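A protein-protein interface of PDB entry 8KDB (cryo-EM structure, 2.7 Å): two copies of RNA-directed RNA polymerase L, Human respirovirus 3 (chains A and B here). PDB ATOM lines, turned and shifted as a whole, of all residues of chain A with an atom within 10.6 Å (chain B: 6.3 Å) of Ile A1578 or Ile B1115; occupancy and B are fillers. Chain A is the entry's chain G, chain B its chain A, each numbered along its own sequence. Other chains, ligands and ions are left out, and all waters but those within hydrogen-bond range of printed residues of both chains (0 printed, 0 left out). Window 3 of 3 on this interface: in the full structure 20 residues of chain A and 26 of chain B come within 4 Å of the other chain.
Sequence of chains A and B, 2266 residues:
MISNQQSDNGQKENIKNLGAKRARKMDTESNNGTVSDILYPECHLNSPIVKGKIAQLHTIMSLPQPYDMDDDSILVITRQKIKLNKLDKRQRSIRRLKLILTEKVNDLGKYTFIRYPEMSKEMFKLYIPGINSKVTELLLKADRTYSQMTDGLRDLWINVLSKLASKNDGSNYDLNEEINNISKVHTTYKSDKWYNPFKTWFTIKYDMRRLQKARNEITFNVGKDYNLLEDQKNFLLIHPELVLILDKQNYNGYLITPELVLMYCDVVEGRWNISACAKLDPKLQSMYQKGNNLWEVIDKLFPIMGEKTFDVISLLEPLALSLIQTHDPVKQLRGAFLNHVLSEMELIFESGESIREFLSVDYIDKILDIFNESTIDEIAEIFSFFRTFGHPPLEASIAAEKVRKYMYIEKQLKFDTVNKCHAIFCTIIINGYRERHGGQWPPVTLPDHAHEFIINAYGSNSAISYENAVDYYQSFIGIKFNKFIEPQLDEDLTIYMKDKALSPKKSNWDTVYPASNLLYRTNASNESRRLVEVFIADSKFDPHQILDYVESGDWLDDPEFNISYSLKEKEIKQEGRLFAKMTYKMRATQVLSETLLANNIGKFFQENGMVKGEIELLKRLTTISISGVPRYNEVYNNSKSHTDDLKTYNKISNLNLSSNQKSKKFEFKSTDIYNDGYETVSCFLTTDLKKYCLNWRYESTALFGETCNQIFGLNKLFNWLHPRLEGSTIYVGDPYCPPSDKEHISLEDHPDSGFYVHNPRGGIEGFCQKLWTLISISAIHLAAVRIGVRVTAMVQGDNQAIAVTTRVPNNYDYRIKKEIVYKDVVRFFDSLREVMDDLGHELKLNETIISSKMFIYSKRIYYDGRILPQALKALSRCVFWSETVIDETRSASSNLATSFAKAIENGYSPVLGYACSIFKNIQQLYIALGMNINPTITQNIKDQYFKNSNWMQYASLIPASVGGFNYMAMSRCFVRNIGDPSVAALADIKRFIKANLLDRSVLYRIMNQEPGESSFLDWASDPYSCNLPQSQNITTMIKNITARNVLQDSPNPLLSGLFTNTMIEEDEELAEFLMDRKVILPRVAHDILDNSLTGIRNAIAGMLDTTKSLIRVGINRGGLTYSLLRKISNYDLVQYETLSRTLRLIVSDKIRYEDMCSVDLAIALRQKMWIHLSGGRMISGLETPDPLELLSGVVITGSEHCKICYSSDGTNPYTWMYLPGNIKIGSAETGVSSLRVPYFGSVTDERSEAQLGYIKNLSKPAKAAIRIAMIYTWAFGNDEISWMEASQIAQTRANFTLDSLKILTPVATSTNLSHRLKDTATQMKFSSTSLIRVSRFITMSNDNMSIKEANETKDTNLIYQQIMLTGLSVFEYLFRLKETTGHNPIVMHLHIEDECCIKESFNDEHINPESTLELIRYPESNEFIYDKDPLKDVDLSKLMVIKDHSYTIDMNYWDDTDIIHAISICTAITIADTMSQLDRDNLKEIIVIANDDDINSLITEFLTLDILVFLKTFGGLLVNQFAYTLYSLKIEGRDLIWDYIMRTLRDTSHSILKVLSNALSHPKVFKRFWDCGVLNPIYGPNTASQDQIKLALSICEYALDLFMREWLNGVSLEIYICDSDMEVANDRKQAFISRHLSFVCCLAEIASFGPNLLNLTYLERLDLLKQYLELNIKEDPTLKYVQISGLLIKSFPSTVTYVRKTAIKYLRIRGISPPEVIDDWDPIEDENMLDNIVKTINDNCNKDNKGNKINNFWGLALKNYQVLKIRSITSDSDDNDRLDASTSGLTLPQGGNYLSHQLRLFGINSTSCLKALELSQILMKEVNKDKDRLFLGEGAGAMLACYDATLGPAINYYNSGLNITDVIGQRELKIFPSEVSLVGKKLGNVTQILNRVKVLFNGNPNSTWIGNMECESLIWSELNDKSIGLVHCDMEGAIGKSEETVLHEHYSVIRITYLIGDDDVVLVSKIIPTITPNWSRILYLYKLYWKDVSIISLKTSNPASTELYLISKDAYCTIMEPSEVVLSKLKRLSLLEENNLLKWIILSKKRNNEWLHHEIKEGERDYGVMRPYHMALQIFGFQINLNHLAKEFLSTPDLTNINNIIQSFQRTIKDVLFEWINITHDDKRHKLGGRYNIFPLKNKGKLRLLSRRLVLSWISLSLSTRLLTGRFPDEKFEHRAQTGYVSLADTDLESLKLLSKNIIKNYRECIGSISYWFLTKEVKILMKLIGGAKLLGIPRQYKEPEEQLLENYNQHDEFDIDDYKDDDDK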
ATOM      1  N   PHE A1566     -21.852 -15.356 -24.861  1.00  0.00           N
ATOM      2  CA  PHE A1566     -22.529 -15.724 -23.624  1.00  0.00           C
ATOM      3  C   PHE A1566     -23.996 -16.031 -23.878  1.00  0.00           C
ATOM      4  O   PHE A1566     -24.539 -16.980 -23.312  1.00  0.00           O
ATOM      5  CB  PHE A1566     -22.387 -14.610 -22.587  1.00  0.00           C
ATOM      6  CG  PHE A1566     -23.054 -14.918 -21.276  1.00  0.00           C
ATOM      7  CD1 PHE A1566     -24.377 -14.575 -21.055  1.00  0.00           C
ATOM      8  CD2 PHE A1566     -22.357 -15.553 -20.265  1.00  0.00           C
ATOM      9  CE1 PHE A1566     -24.991 -14.863 -19.853  1.00  0.00           C
ATOM     10  CE2 PHE A1566     -22.965 -15.842 -19.060  1.00  0.00           C
ATOM     11  CZ  PHE A1566     -24.284 -15.497 -18.854  1.00  0.00           C
ATOM     12  N   TRP A1570     -25.780 -19.519 -23.305  1.00  0.00           N
ATOM     13  CA  TRP A1570     -26.874 -19.450 -22.346  1.00  0.00           C
ATOM     14  C   TRP A1570     -28.133 -20.090 -22.911  1.00  0.00           C
ATOM     15  O   TRP A1570     -28.836 -20.825 -22.209  1.00  0.00           O
ATOM     16  CB  TRP A1570     -27.115 -17.984 -21.985  1.00  0.00           C
ATOM     17  CG  TRP A1570     -28.324 -17.697 -21.162  1.00  0.00           C
ATOM     18  CD1 TRP A1570     -29.590 -17.468 -21.613  1.00  0.00           C
ATOM     19  CD2 TRP A1570     -28.366 -17.525 -19.742  1.00  0.00           C
ATOM     20  NE1 TRP A1570     -30.427 -17.206 -20.557  1.00  0.00           N
ATOM     21  CE2 TRP A1570     -29.698 -17.230 -19.397  1.00  0.00           C
ATOM     22  CE3 TRP A1570     -27.408 -17.611 -18.727  1.00  0.00           C
ATOM     23  CZ2 TRP A1570     -30.096 -17.020 -18.080  1.00  0.00           C
ATOM     24  CZ3 TRP A1570     -27.806 -17.401 -17.422  1.00  0.00           C
ATOM     25  CH2 TRP A1570     -29.137 -17.107 -17.109  1.00  0.00           C
ATOM     26  N   GLY A1573     -27.889 -24.011 -23.232  1.00  0.00           N
ATOM     27  CA  GLY A1573     -28.165 -24.652 -21.963  1.00  0.00           C
ATOM     28  C   GLY A1573     -26.945 -25.037 -21.156  1.00  0.00           C
ATOM     29  O   GLY A1573     -27.100 -25.453 -20.002  1.00  0.00           O
ATOM     30  N   VAL A1574     -25.739 -24.916 -21.716  1.00  0.00           N
ATOM     31  CA  VAL A1574     -24.539 -25.278 -20.967  1.00  0.00           C
ATOM     32  C   VAL A1574     -24.349 -24.347 -19.776  1.00  0.00           C
ATOM     33  O   VAL A1574     -24.020 -24.791 -18.670  1.00  0.00           O
ATOM     34  CB  VAL A1574     -23.309 -25.282 -21.891  1.00  0.00           C
ATOM     35  CG1 VAL A1574     -22.042 -25.486 -21.083  1.00  0.00           C
ATOM     36  CG2 VAL A1574     -23.442 -26.372 -22.938  1.00  0.00           C
ATOM     37  N   LEU A1575     -24.558 -23.047 -19.975  1.00  0.00           N
ATOM     38  CA  LEU A1575     -24.501 -22.080 -18.881  1.00  0.00           C
ATOM     39  C   LEU A1575     -25.864 -22.068 -18.200  1.00  0.00           C
ATOM     40  O   LEU A1575     -26.776 -21.340 -18.591  1.00  0.00           O
ATOM     41  CB  LEU A1575     -24.109 -20.701 -19.393  1.00  0.00           C
ATOM     42  CG  LEU A1575     -22.700 -20.597 -19.982  1.00  0.00           C
ATOM     43  CD1 LEU A1575     -22.462 -19.217 -20.569  1.00  0.00           C
ATOM     44  CD2 LEU A1575     -21.651 -20.929 -18.931  1.00  0.00           C
ATOM     45  N   ASN A1576     -25.998 -22.890 -17.169  1.00  0.00           N
ATOM     46  CA  ASN A1576     -27.283 -23.084 -16.509  1.00  0.00           C
ATOM     47  C   ASN A1576     -27.587 -21.908 -15.588  1.00  0.00           C
ATOM     48  O   ASN A1576     -26.748 -21.548 -14.757  1.00  0.00           O
ATOM     49  CB  ASN A1576     -27.282 -24.383 -15.712  1.00  0.00           C
ATOM     50  CG  ASN A1576     -28.571 -25.161 -15.864  1.00  0.00           C
ATOM     51  OD1 ASN A1576     -29.647 -24.583 -16.005  1.00  0.00           O
ATOM     52  ND2 ASN A1576     -28.468 -26.483 -15.832  1.00  0.00           N
ATOM     53  N   PRO A1577     -28.760 -21.285 -15.713  1.00  0.00           N
ATOM     54  CA  PRO A1577     -29.121 -20.209 -14.776  1.00  0.00           C
ATOM     55  C   PRO A1577     -29.151 -20.653 -13.324  1.00  0.00           C
ATOM     56  O   PRO A1577     -28.850 -19.849 -12.433  1.00  0.00           O
ATOM     57  CB  PRO A1577     -30.516 -19.786 -15.257  1.00  0.00           C
ATOM     58  CG  PRO A1577     -30.569 -20.206 -16.688  1.00  0.00           C
ATOM     59  CD  PRO A1577     -29.759 -21.460 -16.778  1.00  0.00           C
ATOM     60  N   ILE A1578     -29.510 -21.910 -13.061  1.00  0.00           N
ATOM     61  CA  ILE A1578     -29.663 -22.375 -11.686  1.00  0.00           C
ATOM     62  C   ILE A1578     -28.315 -22.465 -10.985  1.00  0.00           C
ATOM     63  O   ILE A1578     -28.190 -22.121  -9.804  1.00  0.00           O
ATOM     64  CB  ILE A1578     -30.389 -23.731 -11.662  1.00  0.00           C
ATOM     65  CG1 ILE A1578     -31.618 -23.699 -12.569  1.00  0.00           C
ATOM     66  CG2 ILE A1578     -30.775 -24.103 -10.242  1.00  0.00           C
ATOM     67  CD1 ILE A1578     -32.169 -25.069 -12.865  1.00  0.00           C
ATOM     68  N   TYR A1579     -27.286 -22.934 -11.694  1.00  0.00           N
ATOM     69  CA  TYR A1579     -26.053 -23.340 -11.027  1.00  0.00           C
ATOM     70  C   TYR A1579     -25.284 -22.154 -10.457  1.00  0.00           C
ATOM     71  O   TYR A1579     -24.408 -22.342  -9.606  1.00  0.00           O
ATOM     72  CB  TYR A1579     -25.179 -24.137 -11.994  1.00  0.00           C
ATOM     73  CG  TYR A1579     -25.771 -25.480 -12.362  1.00  0.00           C
ATOM     74  CD1 TYR A1579     -26.807 -26.030 -11.618  1.00  0.00           C
ATOM     75  CD2 TYR A1579     -25.300 -26.196 -13.454  1.00  0.00           C
ATOM     76  CE1 TYR A1579     -27.355 -27.251 -11.948  1.00  0.00           C
ATOM     77  CE2 TYR A1579     -25.844 -27.421 -13.793  1.00  0.00           C
ATOM     78  CZ  TYR A1579     -26.871 -27.943 -13.036  1.00  0.00           C
ATOM     79  OH  TYR A1579     -27.416 -29.161 -13.367  1.00  0.00           O
ATOM     80  N   GLY A1580     -25.588 -20.939 -10.901  1.00  0.00           N
ATOM     81  CA  GLY A1580     -24.963 -19.762 -10.347  1.00  0.00           C
ATOM     82  C   GLY A1580     -25.381 -18.490 -11.051  1.00  0.00           C
ATOM     83  O   GLY A1580     -25.770 -18.499 -12.223  1.00  0.00           O
ATOM     84  N   PRO A1581     -25.310 -17.360 -10.343  1.00  0.00           N
ATOM     85  CA  PRO A1581     -25.612 -16.073 -10.983  1.00  0.00           C
ATOM     86  C   PRO A1581     -24.456 -15.603 -11.848  1.00  0.00           C
ATOM     87  O   PRO A1581     -23.428 -15.152 -11.330  1.00  0.00           O
ATOM     88  CB  PRO A1581     -25.850 -15.128  -9.796  1.00  0.00           C
ATOM     89  CG  PRO A1581     -25.853 -16.006  -8.559  1.00  0.00           C
ATOM     90  CD  PRO A1581     -25.043 -17.207  -8.906  1.00  0.00           C
ATOM     91  N   ASN A1582     -24.611 -15.698 -13.166  1.00  0.00           N
ATOM     92  CA  ASN A1582     -23.548 -15.365 -14.104  1.00  0.00           C
ATOM     93  C   ASN A1582     -24.107 -14.570 -15.274  1.00  0.00           C
ATOM     94  O   ASN A1582     -25.169 -14.904 -15.810  1.00  0.00           O
ATOM     95  CB  ASN A1582     -22.834 -16.632 -14.597  1.00  0.00           C
ATOM     96  CG  ASN A1582     -23.796 -17.694 -15.105  1.00  0.00           C
ATOM     97  OD1 ASN A1582     -25.009 -17.491 -15.145  1.00  0.00           O
ATOM     98  ND2 ASN A1582     -23.251 -18.841 -15.495  1.00  0.00           N
ATOM     99  N   SER A1594     -16.960 -24.392 -16.244  1.00  0.00           N
ATOM    100  CA  SER A1594     -18.227 -25.066 -16.519  1.00  0.00           C
ATOM    101  C   SER A1594     -18.260 -25.623 -17.938  1.00  0.00           C
ATOM    102  O   SER A1594     -18.737 -26.749 -18.167  1.00  0.00           O
ATOM    103  CB  SER A1594     -19.390 -24.102 -16.292  1.00  0.00           C
ATOM    104  OG  SER A1594     -20.619 -24.681 -16.686  1.00  0.00           O
ATOM    105  N   THR B  34     -36.961 -24.943 -16.990  1.00  0.00           N
ATOM    106  CA  THR B  34     -35.755 -25.354 -16.288  1.00  0.00           C
ATOM    107  C   THR B  34     -35.016 -26.436 -17.067  1.00  0.00           C
ATOM    108  O   THR B  34     -35.612 -27.215 -17.815  1.00  0.00           O
ATOM    109  CB  THR B  34     -36.100 -25.856 -14.885  1.00  0.00           C
ATOM    110  OG1 THR B  34     -34.896 -26.096 -14.149  1.00  0.00           O
ATOM    111  CG2 THR B  34     -36.918 -27.136 -14.953  1.00  0.00           C
ATOM    112  N   VAL B  35     -33.697 -26.465 -16.897  1.00  0.00           N
ATOM    113  CA  VAL B  35     -32.836 -27.441 -17.555  1.00  0.00           C
ATOM    114  C   VAL B  35     -31.996 -28.128 -16.490  1.00  0.00           C
ATOM    115  O   VAL B  35     -31.220 -27.469 -15.787  1.00  0.00           O
ATOM    116  CB  VAL B  35     -31.934 -26.793 -18.618  1.00  0.00           C
ATOM    117  CG1 VAL B  35     -30.875 -27.776 -19.082  1.00  0.00           C
ATOM    118  CG2 VAL B  35     -32.765 -26.312 -19.793  1.00  0.00           C
ATOM    119  N   SER B  36     -32.150 -29.443 -16.371  1.00  0.00           N
ATOM    120  CA  SER B  36     -31.325 -30.232 -15.468  1.00  0.00           C
ATOM    121  C   SER B  36     -31.375 -31.682 -15.919  1.00  0.00           C
ATOM    122  O   SER B  36     -32.327 -32.116 -16.573  1.00  0.00           O
ATOM    123  CB  SER B  36     -31.787 -30.098 -14.013  1.00  0.00           C
ATOM    124  OG  SER B  36     -30.934 -30.821 -13.145  1.00  0.00           O
ATOM    125  N   LEU B1110     -36.079 -30.773  -4.819  1.00  0.00           N
ATOM    126  CA  LEU B1110     -34.713 -30.299  -4.633  1.00  0.00           C
ATOM    127  C   LEU B1110     -34.374 -29.195  -5.622  1.00  0.00           C
ATOM    128  O   LEU B1110     -33.789 -28.176  -5.246  1.00  0.00           O
ATOM    129  CB  LEU B1110     -33.727 -31.458  -4.771  1.00  0.00           C
ATOM    130  CG  LEU B1110     -32.250 -31.068  -4.722  1.00  0.00           C
ATOM    131  CD1 LEU B1110     -31.816 -30.778  -3.297  1.00  0.00           C
ATOM    132  CD2 LEU B1110     -31.391 -32.157  -5.332  1.00  0.00           C
ATOM    133  N   ILE B1111     -34.754 -29.370  -6.888  1.00  0.00           N
ATOM    134  CA  ILE B1111     -34.485 -28.345  -7.890  1.00  0.00           C
ATOM    135  C   ILE B1111     -35.252 -27.069  -7.574  1.00  0.00           C
ATOM    136  O   ILE B1111     -34.707 -25.964  -7.676  1.00  0.00           O
ATOM    137  CB  ILE B1111     -34.811 -28.877  -9.296  1.00  0.00           C
ATOM    138  CG1 ILE B1111     -33.756 -29.892  -9.733  1.00  0.00           C
ATOM    139  CG2 ILE B1111     -34.894 -27.738 -10.297  1.00  0.00           C
ATOM    140  CD1 ILE B1111     -32.368 -29.308  -9.860  1.00  0.00           C
ATOM    141  N   ARG B1112     -36.522 -27.193  -7.179  1.00  0.00           N
ATOM    142  CA  ARG B1112     -37.314 -26.003  -6.876  1.00  0.00           C
ATOM    143  C   ARG B1112     -36.731 -25.231  -5.695  1.00  0.00           C
ATOM    144  O   ARG B1112     -36.576 -24.003  -5.753  1.00  0.00           O
ATOM    145  CB  ARG B1112     -38.766 -26.398  -6.605  1.00  0.00           C
ATOM    146  CG  ARG B1112     -39.578 -25.326  -5.909  1.00  0.00           C
ATOM    147  CD  ARG B1112     -41.047 -25.702  -5.823  1.00  0.00           C
ATOM    148  NE  ARG B1112     -41.240 -27.081  -5.393  1.00  0.00           N
ATOM    149  CZ  ARG B1112     -41.240 -27.480  -4.130  1.00  0.00           C
ATOM    150  NH1 ARG B1112     -41.041 -26.630  -3.136  1.00  0.00           N
ATOM    151  NH2 ARG B1112     -41.445 -28.765  -3.855  1.00  0.00           N
ATOM    152  N   VAL B1113     -36.383 -25.936  -4.618  1.00  0.00           N
ATOM    153  CA  VAL B1113     -35.840 -25.266  -3.441  1.00  0.00           C
ATOM    154  C   VAL B1113     -34.459 -24.691  -3.735  1.00  0.00           C
ATOM    155  O   VAL B1113     -34.099 -23.623  -3.226  1.00  0.00           O
ATOM    156  CB  VAL B1113     -35.821 -26.223  -2.237  1.00  0.00           C
ATOM    157  CG1 VAL B1113     -35.280 -25.518  -1.012  1.00  0.00           C
ATOM    158  CG2 VAL B1113     -37.218 -26.740  -1.954  1.00  0.00           C
ATOM    159  N   GLY B1114     -33.662 -25.381  -4.554  1.00  0.00           N
ATOM    160  CA  GLY B1114     -32.370 -24.839  -4.934  1.00  0.00           C
ATOM    161  C   GLY B1114     -32.490 -23.591  -5.785  1.00  0.00           C
ATOM    162  O   GLY B1114     -31.675 -22.673  -5.674  1.00  0.00           O
ATOM    163  N   ILE B1115     -33.497 -23.543  -6.656  1.00  0.00           N
ATOM    164  CA  ILE B1115     -33.768 -22.314  -7.397  1.00  0.00           C
ATOM    165  C   ILE B1115     -34.159 -21.200  -6.437  1.00  0.00           C
ATOM    166  O   ILE B1115     -33.703 -20.058  -6.566  1.00  0.00           O
ATOM    167  CB  ILE B1115     -34.857 -22.557  -8.459  1.00  0.00           C
ATOM    168  CG1 ILE B1115     -34.302 -23.388  -9.614  1.00  0.00           C
ATOM    169  CG2 ILE B1115     -35.402 -21.240  -8.976  1.00  0.00           C
ATOM    170  CD1 ILE B1115     -35.301 -23.623 -10.724  1.00  0.00           C
ATOM    171  N   ASN B1116     -35.002 -21.520  -5.452  1.00  0.00           N
ATOM    172  CA  ASN B1116     -35.457 -20.504  -4.507  1.00  0.00           C
ATOM    173  C   ASN B1116     -34.309 -19.960  -3.662  1.00  0.00           C
ATOM    174  O   ASN B1116     -34.247 -18.755  -3.393  1.00  0.00           O
ATOM    175  CB  ASN B1116     -36.556 -21.080  -3.613  1.00  0.00           C
ATOM    176  CG  ASN B1116     -37.262 -20.014  -2.798  1.00  0.00           C
ATOM    177  OD1 ASN B1116     -36.696 -19.456  -1.858  1.00  0.00           O
ATOM    178  ND2 ASN B1116     -38.506 -19.724  -3.157  1.00  0.00           N
ATOM    179  N   ARG B1117     -33.391 -20.826  -3.235  1.00  0.00           N
ATOM    180  CA  ARG B1117     -32.347 -20.446  -2.289  1.00  0.00           C
ATOM    181  C   ARG B1117     -30.952 -20.367  -2.887  1.00  0.00           C
ATOM    182  O   ARG B1117     -30.119 -19.623  -2.366  1.00  0.00           O
ATOM    183  CB  ARG B1117     -32.313 -21.429  -1.112  1.00  0.00           C
ATOM    184  CG  ARG B1117     -33.667 -21.718  -0.498  1.00  0.00           C
ATOM    185  CD  ARG B1117     -34.123 -20.566   0.374  1.00  0.00           C
ATOM    186  NE  ARG B1117     -33.029 -20.043   1.185  1.00  0.00           N
ATOM    187  CZ  ARG B1117     -33.107 -18.953   1.935  1.00  0.00           C
ATOM    188  NH1 ARG B1117     -34.222 -18.247   2.015  1.00  0.00           N
ATOM    189  NH2 ARG B1117     -32.038 -18.564   2.623  1.00  0.00           N
ATOM    190  N   GLY B1118     -30.666 -21.107  -3.953  1.00  0.00           N
ATOM    191  CA  GLY B1118     -29.324 -21.156  -4.497  1.00  0.00           C
ATOM    192  C   GLY B1118     -28.458 -22.193  -3.811  1.00  0.00           C
ATOM    193  O   GLY B1118     -28.846 -22.850  -2.842  1.00  0.00           O
ATOM    194  N   GLY B1119     -27.242 -22.339  -4.337  1.00  0.00           N
ATOM    195  CA  GLY B1119     -26.266 -23.255  -3.787  1.00  0.00           C
ATOM    196  C   GLY B1119     -26.026 -24.511  -4.597  1.00  0.00           C
ATOM    197  O   GLY B1119     -25.095 -25.261  -4.278  1.00  0.00           O
ATOM    198  N   LEU B1120     -26.829 -24.769  -5.626  1.00  0.00           N
ATOM    199  CA  LEU B1120     -26.640 -25.950  -6.455  1.00  0.00           C
ATOM    200  C   LEU B1120     -25.572 -25.700  -7.512  1.00  0.00           C
ATOM    201  O   LEU B1120     -25.303 -24.558  -7.898  1.00  0.00           O
ATOM    202  CB  LEU B1120     -27.953 -26.352  -7.126  1.00  0.00           C
ATOM    203  CG  LEU B1120     -29.095 -26.772  -6.201  1.00  0.00           C
ATOM    204  CD1 LEU B1120     -30.312 -27.184  -7.006  1.00  0.00           C
ATOM    205  CD2 LEU B1120     -28.656 -27.893  -5.279  1.00  0.00           C
ATOM    206  N   THR B1121     -24.959 -26.784  -7.983  1.00  0.00           N
ATOM    207  CA  THR B1121     -23.929 -26.694  -9.008  1.00  0.00           C
ATOM    208  C   THR B1121     -23.892 -27.990  -9.805  1.00  0.00           C
ATOM    209  O   THR B1121     -24.415 -29.021  -9.378  1.00  0.00           O
ATOM    210  CB  THR B1121     -22.553 -26.394  -8.403  1.00  0.00           C
ATOM    211  OG1 THR B1121     -21.561 -26.415  -9.437  1.00  0.00           O
ATOM    212  CG2 THR B1121     -22.198 -27.422  -7.348  1.00  0.00           C
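ND2 of Asn A1576 sits at hydrogen-bond distance from O of Val B35.
O of Leu B1120 lies close to O of Tyr A1579.
Among the printed residues, pairs that only touch across the chains: Ile A1578 with Thr B34, Ile A1578 with Val B35, Ile A1578 with Ile B1115, Tyr A1579 with Ser B36 and Tyr A1579 with Thr B1121.
Pro A1577 touches none of the printed residues of chain B.
Of the printed residues of chain B, Ile A1578 touches Thr B34, Val B35 and Ile B1115.
Of the printed residues of chain B, Tyr A1579 touches Ser B36, Leu B1120 and Thr B1121.
Thr B34 touches just one residue of chain A: Ile A1578 (3.2 Å).
Val B1113 touches none of the printed residues of chain A.
Of the printed residues of chain A, Ile B1115 touches Ile A1578 (3.7 Å).
No residue of chain A comes within 4 Å of Asn B1116.
Printed residues of chain A within 4 Å of Thr B1121: Tyr A1579.
The nearest residue of chain B that does not touch Ile A1578 is Leu B1120 (4.2 Å).
Of the 13 printed residues of chain A, 3 touch a printed residue of chain B.
Hydrophobic or aromatic side chains of chain A within 4 Å of the printed part of chain B: Ile A1578 and Tyr A1579.
Along chain A the printed residues that touch a printed residue of chain B span positions 1576 to 1579.
Of the 15 printed residues of chain B, 6 touch a printed residue of chain A.
Hydrophobic or aromatic side chains of chain B within 4 Å of the printed part of chain A: Ile B1115.
Among the printed residues, 7 pairs touch across the chains.
Among the printed residues, no Asp or Glu carboxylate lies within 4 Å of a Lys or Arg side-chain nitrogen of the other chain.
No position is printed for both chains.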
